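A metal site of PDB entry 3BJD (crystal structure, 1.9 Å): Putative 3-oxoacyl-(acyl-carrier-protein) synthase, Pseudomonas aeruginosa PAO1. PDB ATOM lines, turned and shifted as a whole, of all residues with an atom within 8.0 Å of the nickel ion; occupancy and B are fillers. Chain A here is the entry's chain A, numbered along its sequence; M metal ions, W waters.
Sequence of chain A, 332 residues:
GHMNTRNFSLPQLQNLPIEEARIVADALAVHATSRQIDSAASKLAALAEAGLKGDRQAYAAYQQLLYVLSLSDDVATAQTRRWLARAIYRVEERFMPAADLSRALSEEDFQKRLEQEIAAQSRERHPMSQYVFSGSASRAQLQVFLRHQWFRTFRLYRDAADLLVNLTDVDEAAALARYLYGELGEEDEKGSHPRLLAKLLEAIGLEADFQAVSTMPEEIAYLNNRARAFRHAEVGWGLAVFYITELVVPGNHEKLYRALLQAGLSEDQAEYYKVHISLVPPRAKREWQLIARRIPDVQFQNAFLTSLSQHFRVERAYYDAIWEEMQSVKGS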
ATOM      1  N   THR A 153       4.413   2.451  -4.657  1.00  0.00           N
ATOM      2  CA  THR A 153       3.556   1.867  -5.694  1.00  0.00           C
ATOM      3  C   THR A 153       4.168   1.778  -7.077  1.00  0.00           C
ATOM      4  O   THR A 153       3.962   0.785  -7.792  1.00  0.00           O
ATOM      5  CB  THR A 153       2.254   2.697  -5.810  1.00  0.00           C
ATOM      6  OG1 THR A 153       1.508   2.538  -4.604  1.00  0.00           O
ATOM      7  CG2 THR A 153       1.341   2.243  -6.981  1.00  0.00           C
ATOM      8  N   LEU A 156       6.239  -1.304  -7.985  1.00  0.00           N
ATOM      9  CA  LEU A 156       5.978  -2.574  -7.289  1.00  0.00           C
ATOM     10  C   LEU A 156       5.867  -3.754  -8.264  1.00  0.00           C
ATOM     11  O   LEU A 156       6.388  -4.852  -8.019  1.00  0.00           O
ATOM     12  CB  LEU A 156       4.712  -2.474  -6.435  1.00  0.00           C
ATOM     13  CG  LEU A 156       4.336  -3.755  -5.678  1.00  0.00           C
ATOM     14  CD1 LEU A 156       5.486  -4.351  -4.786  1.00  0.00           C
ATOM     15  CD2 LEU A 156       3.053  -3.486  -4.836  1.00  0.00           C
ATOM     16  N   TYR A 157       5.210  -3.531  -9.400  1.00  0.00           N
ATOM     17  CA  TYR A 157       4.986  -4.613 -10.377  1.00  0.00           C
ATOM     18  C   TYR A 157       6.322  -5.246 -10.828  1.00  0.00           C
ATOM     19  O   TYR A 157       6.391  -6.436 -11.160  1.00  0.00           O
ATOM     20  CB  TYR A 157       4.163  -4.064 -11.580  1.00  0.00           C
ATOM     21  CG  TYR A 157       4.959  -3.130 -12.489  1.00  0.00           C
ATOM     22  CD1 TYR A 157       5.683  -3.628 -13.580  1.00  0.00           C
ATOM     23  CD2 TYR A 157       4.973  -1.750 -12.252  1.00  0.00           C
ATOM     24  CE1 TYR A 157       6.389  -2.793 -14.416  1.00  0.00           C
ATOM     25  CE2 TYR A 157       5.706  -0.892 -13.079  1.00  0.00           C
ATOM     26  CZ  TYR A 157       6.408  -1.428 -14.135  1.00  0.00           C
ATOM     27  OH  TYR A 157       7.102  -0.581 -14.931  1.00  0.00           O
ATOM     28  N   TYR A 179      -1.476 -11.821 -11.237  1.00  0.00           N
ATOM     29  CA  TYR A 179      -1.223 -10.623 -10.411  1.00  0.00           C
ATOM     30  C   TYR A 179      -0.761  -9.484 -11.306  1.00  0.00           C
ATOM     31  O   TYR A 179      -1.303  -8.385 -11.226  1.00  0.00           O
ATOM     32  CB  TYR A 179      -0.154 -10.890  -9.338  1.00  0.00           C
ATOM     33  CG  TYR A 179       0.276  -9.624  -8.618  1.00  0.00           C
ATOM     34  CD1 TYR A 179      -0.458  -9.140  -7.525  1.00  0.00           C
ATOM     35  CD2 TYR A 179       1.402  -8.897  -9.041  1.00  0.00           C
ATOM     36  CE1 TYR A 179      -0.080  -7.964  -6.878  1.00  0.00           C
ATOM     37  CE2 TYR A 179       1.786  -7.711  -8.402  1.00  0.00           C
ATOM     38  CZ  TYR A 179       1.038  -7.268  -7.316  1.00  0.00           C
ATOM     39  OH  TYR A 179       1.423  -6.124  -6.641  1.00  0.00           O
ATOM     40  N   GLY A 182      -3.446  -7.876 -13.627  1.00  0.00           N
ATOM     41  CA  GLY A 182      -4.338  -6.952 -12.934  1.00  0.00           C
ATOM     42  C   GLY A 182      -3.614  -5.662 -12.573  1.00  0.00           C
ATOM     43  O   GLY A 182      -4.150  -4.565 -12.783  1.00  0.00           O
ATOM     44  N   GLU A 183      -2.391  -5.782 -12.032  1.00  0.00           N
ATOM     45  CA  GLU A 183      -1.593  -4.628 -11.622  1.00  0.00           C
ATOM     46  C   GLU A 183      -1.276  -3.660 -12.800  1.00  0.00           C
ATOM     47  O   GLU A 183      -1.156  -2.436 -12.614  1.00  0.00           O
ATOM     48  CB  GLU A 183      -0.288  -5.110 -10.981  1.00  0.00           C
ATOM     49  CG  GLU A 183       0.574  -4.012 -10.342  1.00  0.00           C
ATOM     50  CD  GLU A 183      -0.054  -3.361  -9.085  1.00  0.00           C
ATOM     51  OE1 GLU A 183      -1.049  -3.929  -8.534  1.00  0.00           O
ATOM     52  OE2 GLU A 183       0.486  -2.304  -8.660  1.00  0.00           O
ATOM     53  N   LEU A 184      -1.175  -4.204 -14.001  1.00  0.00           N
ATOM     54  CA  LEU A 184      -0.838  -3.387 -15.180  1.00  0.00           C
ATOM     55  C   LEU A 184      -2.009  -3.020 -16.068  1.00  0.00           C
ATOM     56  O   LEU A 184      -1.804  -2.666 -17.235  1.00  0.00           O
ATOM     57  CB  LEU A 184       0.277  -4.049 -16.004  1.00  0.00           C
ATOM     58  CG  LEU A 184       1.631  -3.997 -15.277  1.00  0.00           C
ATOM     59  CD1 LEU A 184       2.622  -4.968 -15.910  1.00  0.00           C
ATOM     60  CD2 LEU A 184       2.219  -2.586 -15.233  1.00  0.00           C
ATOM     61  N   GLY A 191      -5.023   2.078 -17.443  1.00  0.00           N
ATOM     62  CA  GLY A 191      -5.501   1.686 -16.131  1.00  0.00           C
ATOM     63  C   GLY A 191      -4.519   0.918 -15.259  1.00  0.00           C
ATOM     64  O   GLY A 191      -4.900   0.402 -14.218  1.00  0.00           O
ATOM     65  N   SER A 192      -3.270   0.813 -15.669  1.00  0.00           N
ATOM     66  CA  SER A 192      -2.224   0.266 -14.770  1.00  0.00           C
ATOM     67  C   SER A 192      -2.242   0.986 -13.421  1.00  0.00           C
ATOM     68  O   SER A 192      -2.520   2.177 -13.344  1.00  0.00           O
ATOM     69  CB  SER A 192      -0.820   0.307 -15.411  1.00  0.00           C
ATOM     70  OG  SER A 192      -0.262   1.634 -15.443  1.00  0.00           O
ATOM     71  N   HIS A 193      -1.944   0.265 -12.352  1.00  0.00           N
ATOM     72  CA  HIS A 193      -1.998   0.872 -11.032  1.00  0.00           C
ATOM     73  C   HIS A 193      -1.059   2.081 -10.844  1.00  0.00           C
ATOM     74  O   HIS A 193      -1.461   3.076 -10.212  1.00  0.00           O
ATOM     75  CB  HIS A 193      -1.930  -0.217  -9.948  1.00  0.00           C
ATOM     76  CG  HIS A 193      -3.124  -1.131  -9.989  1.00  0.00           C
ATOM     77  ND1 HIS A 193      -3.350  -2.117  -9.063  1.00  0.00           N
ATOM     78  CD2 HIS A 193      -4.168  -1.171 -10.843  1.00  0.00           C
ATOM     79  CE1 HIS A 193      -4.469  -2.750  -9.354  1.00  0.00           C
ATOM     80  NE2 HIS A 193      -4.997  -2.191 -10.426  1.00  0.00           N
ATOM     81  N   PRO A 194       0.168   2.023 -11.399  1.00  0.00           N
ATOM     82  CA  PRO A 194       0.992   3.234 -11.338  1.00  0.00           C
ATOM     83  C   PRO A 194       0.306   4.405 -12.024  1.00  0.00           C
ATOM     84  O   PRO A 194       0.323   5.514 -11.487  1.00  0.00           O
ATOM     85  CB  PRO A 194       2.292   2.816 -12.090  1.00  0.00           C
ATOM     86  CG  PRO A 194       2.392   1.287 -11.784  1.00  0.00           C
ATOM     87  CD  PRO A 194       0.916   0.908 -12.037  1.00  0.00           C
ATOM     88  N   LEU A 196      -2.986   4.894 -12.513  1.00  0.00           N
ATOM     89  CA  LEU A 196      -4.090   5.267 -11.604  1.00  0.00           C
ATOM     90  C   LEU A 196      -3.578   6.193 -10.484  1.00  0.00           C
ATOM     91  O   LEU A 196      -4.175   7.264 -10.211  1.00  0.00           O
ATOM     92  CB  LEU A 196      -4.791   4.017 -11.023  1.00  0.00           C
ATOM     93  CG  LEU A 196      -5.523   3.134 -12.037  1.00  0.00           C
ATOM     94  CD1 LEU A 196      -6.347   2.075 -11.221  1.00  0.00           C
ATOM     95  CD2 LEU A 196      -6.515   3.965 -12.939  1.00  0.00           C
ATOM     96  N   THR A 245       1.791  -7.666   1.776  1.00  0.00           N
ATOM     97  CA  THR A 245       1.262  -6.588   0.935  1.00  0.00           C
ATOM     98  C   THR A 245      -0.154  -6.911   0.443  1.00  0.00           C
ATOM     99  O   THR A 245      -1.051  -6.065   0.558  1.00  0.00           O
ATOM    100  CB  THR A 245       2.169  -6.261  -0.283  1.00  0.00           C
ATOM    101  OG1 THR A 245       3.440  -5.769   0.182  1.00  0.00           O
ATOM    102  CG2 THR A 245       1.542  -5.181  -1.184  1.00  0.00           C
ATOM    103  N   GLU A 246      -0.356  -8.100  -0.094  1.00  0.00           N
ATOM    104  CA  GLU A 246      -1.682  -8.517  -0.583  1.00  0.00           C
ATOM    105  C   GLU A 246      -2.727  -8.593   0.530  1.00  0.00           C
ATOM    106  O   GLU A 246      -3.889  -8.244   0.313  1.00  0.00           O
ATOM    107  CB  GLU A 246      -1.593  -9.846  -1.328  1.00  0.00           C
ATOM    108  CG  GLU A 246      -0.931  -9.741  -2.711  1.00  0.00           C
ATOM    109  CD  GLU A 246      -1.870  -9.195  -3.778  1.00  0.00           C
ATOM    110  OE1 GLU A 246      -2.510 -10.018  -4.491  1.00  0.00           O
ATOM    111  OE2 GLU A 246      -2.009  -7.945  -3.910  1.00  0.00           O
ATOM    112  N   VAL A 249      -3.257  -4.433   2.063  1.00  0.00           N
ATOM    113  CA  VAL A 249      -3.696  -3.407   1.080  1.00  0.00           C
ATOM    114  C   VAL A 249      -5.230  -3.142   0.939  1.00  0.00           C
ATOM    115  O   VAL A 249      -5.654  -1.975   0.987  1.00  0.00           O
ATOM    116  CB  VAL A 249      -2.994  -3.591  -0.301  1.00  0.00           C
ATOM    117  CG1 VAL A 249      -3.683  -2.779  -1.400  1.00  0.00           C
ATOM    118  CG2 VAL A 249      -1.521  -3.222  -0.184  1.00  0.00           C
ATOM    119  N   HIS A 253      -6.439   0.602   1.882  1.00  0.00           N
ATOM    120  CA  HIS A 253      -6.898   1.279   0.687  1.00  0.00           C
ATOM    121  C   HIS A 253      -8.365   1.726   0.725  1.00  0.00           C
ATOM    122  O   HIS A 253      -8.693   2.767   0.164  1.00  0.00           O
ATOM    123  CB  HIS A 253      -6.590   0.412  -0.553  1.00  0.00           C
ATOM    124  CG  HIS A 253      -5.170   0.536  -1.030  1.00  0.00           C
ATOM    125  ND1 HIS A 253      -4.096   0.555  -0.168  1.00  0.00           N
ATOM    126  CD2 HIS A 253      -4.656   0.618  -2.273  1.00  0.00           C
ATOM    127  CE1 HIS A 253      -2.977   0.665  -0.862  1.00  0.00           C
ATOM    128  NE2 HIS A 253      -3.290   0.700  -2.145  1.00  0.00           N
ATOM    129  N   TYR A 272      -7.462   4.722  -7.820  1.00  0.00           N
ATOM    130  CA  TYR A 272      -6.318   3.927  -7.330  1.00  0.00           C
ATOM    131  C   TYR A 272      -6.647   3.158  -6.040  1.00  0.00           C
ATOM    132  O   TYR A 272      -6.329   1.969  -5.921  1.00  0.00           O
ATOM    133  CB  TYR A 272      -5.025   4.780  -7.156  1.00  0.00           C
ATOM    134  CG  TYR A 272      -3.939   3.980  -6.497  1.00  0.00           C
ATOM    135  CD1 TYR A 272      -3.180   3.042  -7.233  1.00  0.00           C
ATOM    136  CD2 TYR A 272      -3.718   4.073  -5.104  1.00  0.00           C
ATOM    137  CE1 TYR A 272      -2.226   2.264  -6.613  1.00  0.00           C
ATOM    138  CE2 TYR A 272      -2.724   3.287  -4.478  1.00  0.00           C
ATOM    139  CZ  TYR A 272      -1.988   2.385  -5.247  1.00  0.00           C
ATOM    140  OH  TYR A 272      -1.013   1.573  -4.671  1.00  0.00           O
ATOM    141  N   VAL A 275      -9.877   0.451  -6.485  1.00  0.00           N
ATOM    142  CA  VAL A 275      -9.687  -0.806  -7.214  1.00  0.00           C
ATOM    143  C   VAL A 275      -9.112  -1.940  -6.380  1.00  0.00           C
ATOM    144  O   VAL A 275      -9.316  -3.115  -6.714  1.00  0.00           O
ATOM    145  CB  VAL A 275      -8.902  -0.661  -8.565  1.00  0.00           C
ATOM    146  CG1 VAL A 275      -9.613   0.313  -9.498  1.00  0.00           C
ATOM    147  CG2 VAL A 275      -7.457  -0.268  -8.341  1.00  0.00           C
ATOM    148  N   HIS A 276      -8.425  -1.593  -5.298  1.00  0.00           N
ATOM    149  CA  HIS A 276      -7.812  -2.570  -4.409  1.00  0.00           C
ATOM    150  C   HIS A 276      -8.767  -3.204  -3.387  1.00  0.00           C
ATOM    151  O   HIS A 276      -8.635  -4.387  -3.056  1.00  0.00           O
ATOM    152  CB  HIS A 276      -6.590  -1.950  -3.729  1.00  0.00           C
ATOM    153  CG  HIS A 276      -5.475  -1.709  -4.680  1.00  0.00           C
ATOM    154  ND1 HIS A 276      -5.310  -0.502  -5.347  1.00  0.00           N
ATOM    155  CD2 HIS A 276      -4.496  -2.532  -5.132  1.00  0.00           C
ATOM    156  CE1 HIS A 276      -4.259  -0.590  -6.145  1.00  0.00           C
ATOM    157  NE2 HIS A 276      -3.738  -1.806  -6.026  1.00  0.00           N
ATOM    158  N   LEU A 279     -10.207  -5.966  -6.199  1.00  0.00           N
ATOM    159  CA  LEU A 279      -9.486  -7.027  -6.931  1.00  0.00           C
ATOM    160  C   LEU A 279      -8.630  -7.957  -6.085  1.00  0.00           C
ATOM    161  O   LEU A 279      -8.396  -9.103  -6.489  1.00  0.00           O
ATOM    162  CB  LEU A 279      -8.675  -6.476  -8.132  1.00  0.00           C
ATOM    163  CG  LEU A 279      -7.405  -5.604  -8.086  1.00  0.00           C
ATOM    164  CD1 LEU A 279      -6.228  -6.209  -7.322  1.00  0.00           C
ATOM    165  CD2 LEU A 279      -6.994  -5.266  -9.509  1.00  0.00           C
ATOM    166  N   VAL A 280      -8.156  -7.490  -4.933  1.00  0.00           N
ATOM    167  CA  VAL A 280      -7.187  -8.279  -4.158  1.00  0.00           C
ATOM    168  C   VAL A 280      -7.765  -9.348  -3.196  1.00  0.00           C
ATOM    169  O   VAL A 280      -7.231 -10.459  -3.160  1.00  0.00           O
ATOM    170  CB  VAL A 280      -5.974  -7.425  -3.585  1.00  0.00           C
ATOM    171  CG1 VAL A 280      -6.408  -6.043  -3.083  1.00  0.00           C
ATOM    172  CG2 VAL A 280      -5.157  -8.186  -2.541  1.00  0.00           C
HETATM  173 NI    NI M   1      -2.276  -2.607  -7.380  1.00  0.00          NI
HETATM  174  O   HOH W   1      -2.952  -5.046  -7.953  1.00  0.00           O
HETATM  175  O   HOH W   2      -0.769  -1.099  -6.885  1.00  0.00           O
HETATM  176  O   HOH W   3      -1.196  -3.448  -5.401  1.00  0.00           O
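NE2 of His 193 is in hydrogen-bond range of O of Gly 182 (3.5 Å). A ring nitrogen (ND1) of His 276 sits at hydrogen-bond distance from the backbone carbonyl oxygen (O) of Tyr 272, 2.7 Å away.
Three residues have an atom within 4 Å of the nickel ion: Glu 183, His 193 and His 276. The nearest printed residue that does not touch the nickel ion is Tyr 272 (4.9 Å).
The nickel ion is bound by ND1 of His 193 (2.1 Å), OE1 of Glu 183 (2.1 Å), NE2 of His 276 (2.1 Å), water W2 (2.2 Å), water W3 (2.4 Å) and water W1 (2.6 Å). The nickel ion has six donor atoms within binding distance.
Water W2 bridges OE2 of Glu 183 (2.5 Å) and OH of Tyr 272 (3.5 Å).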
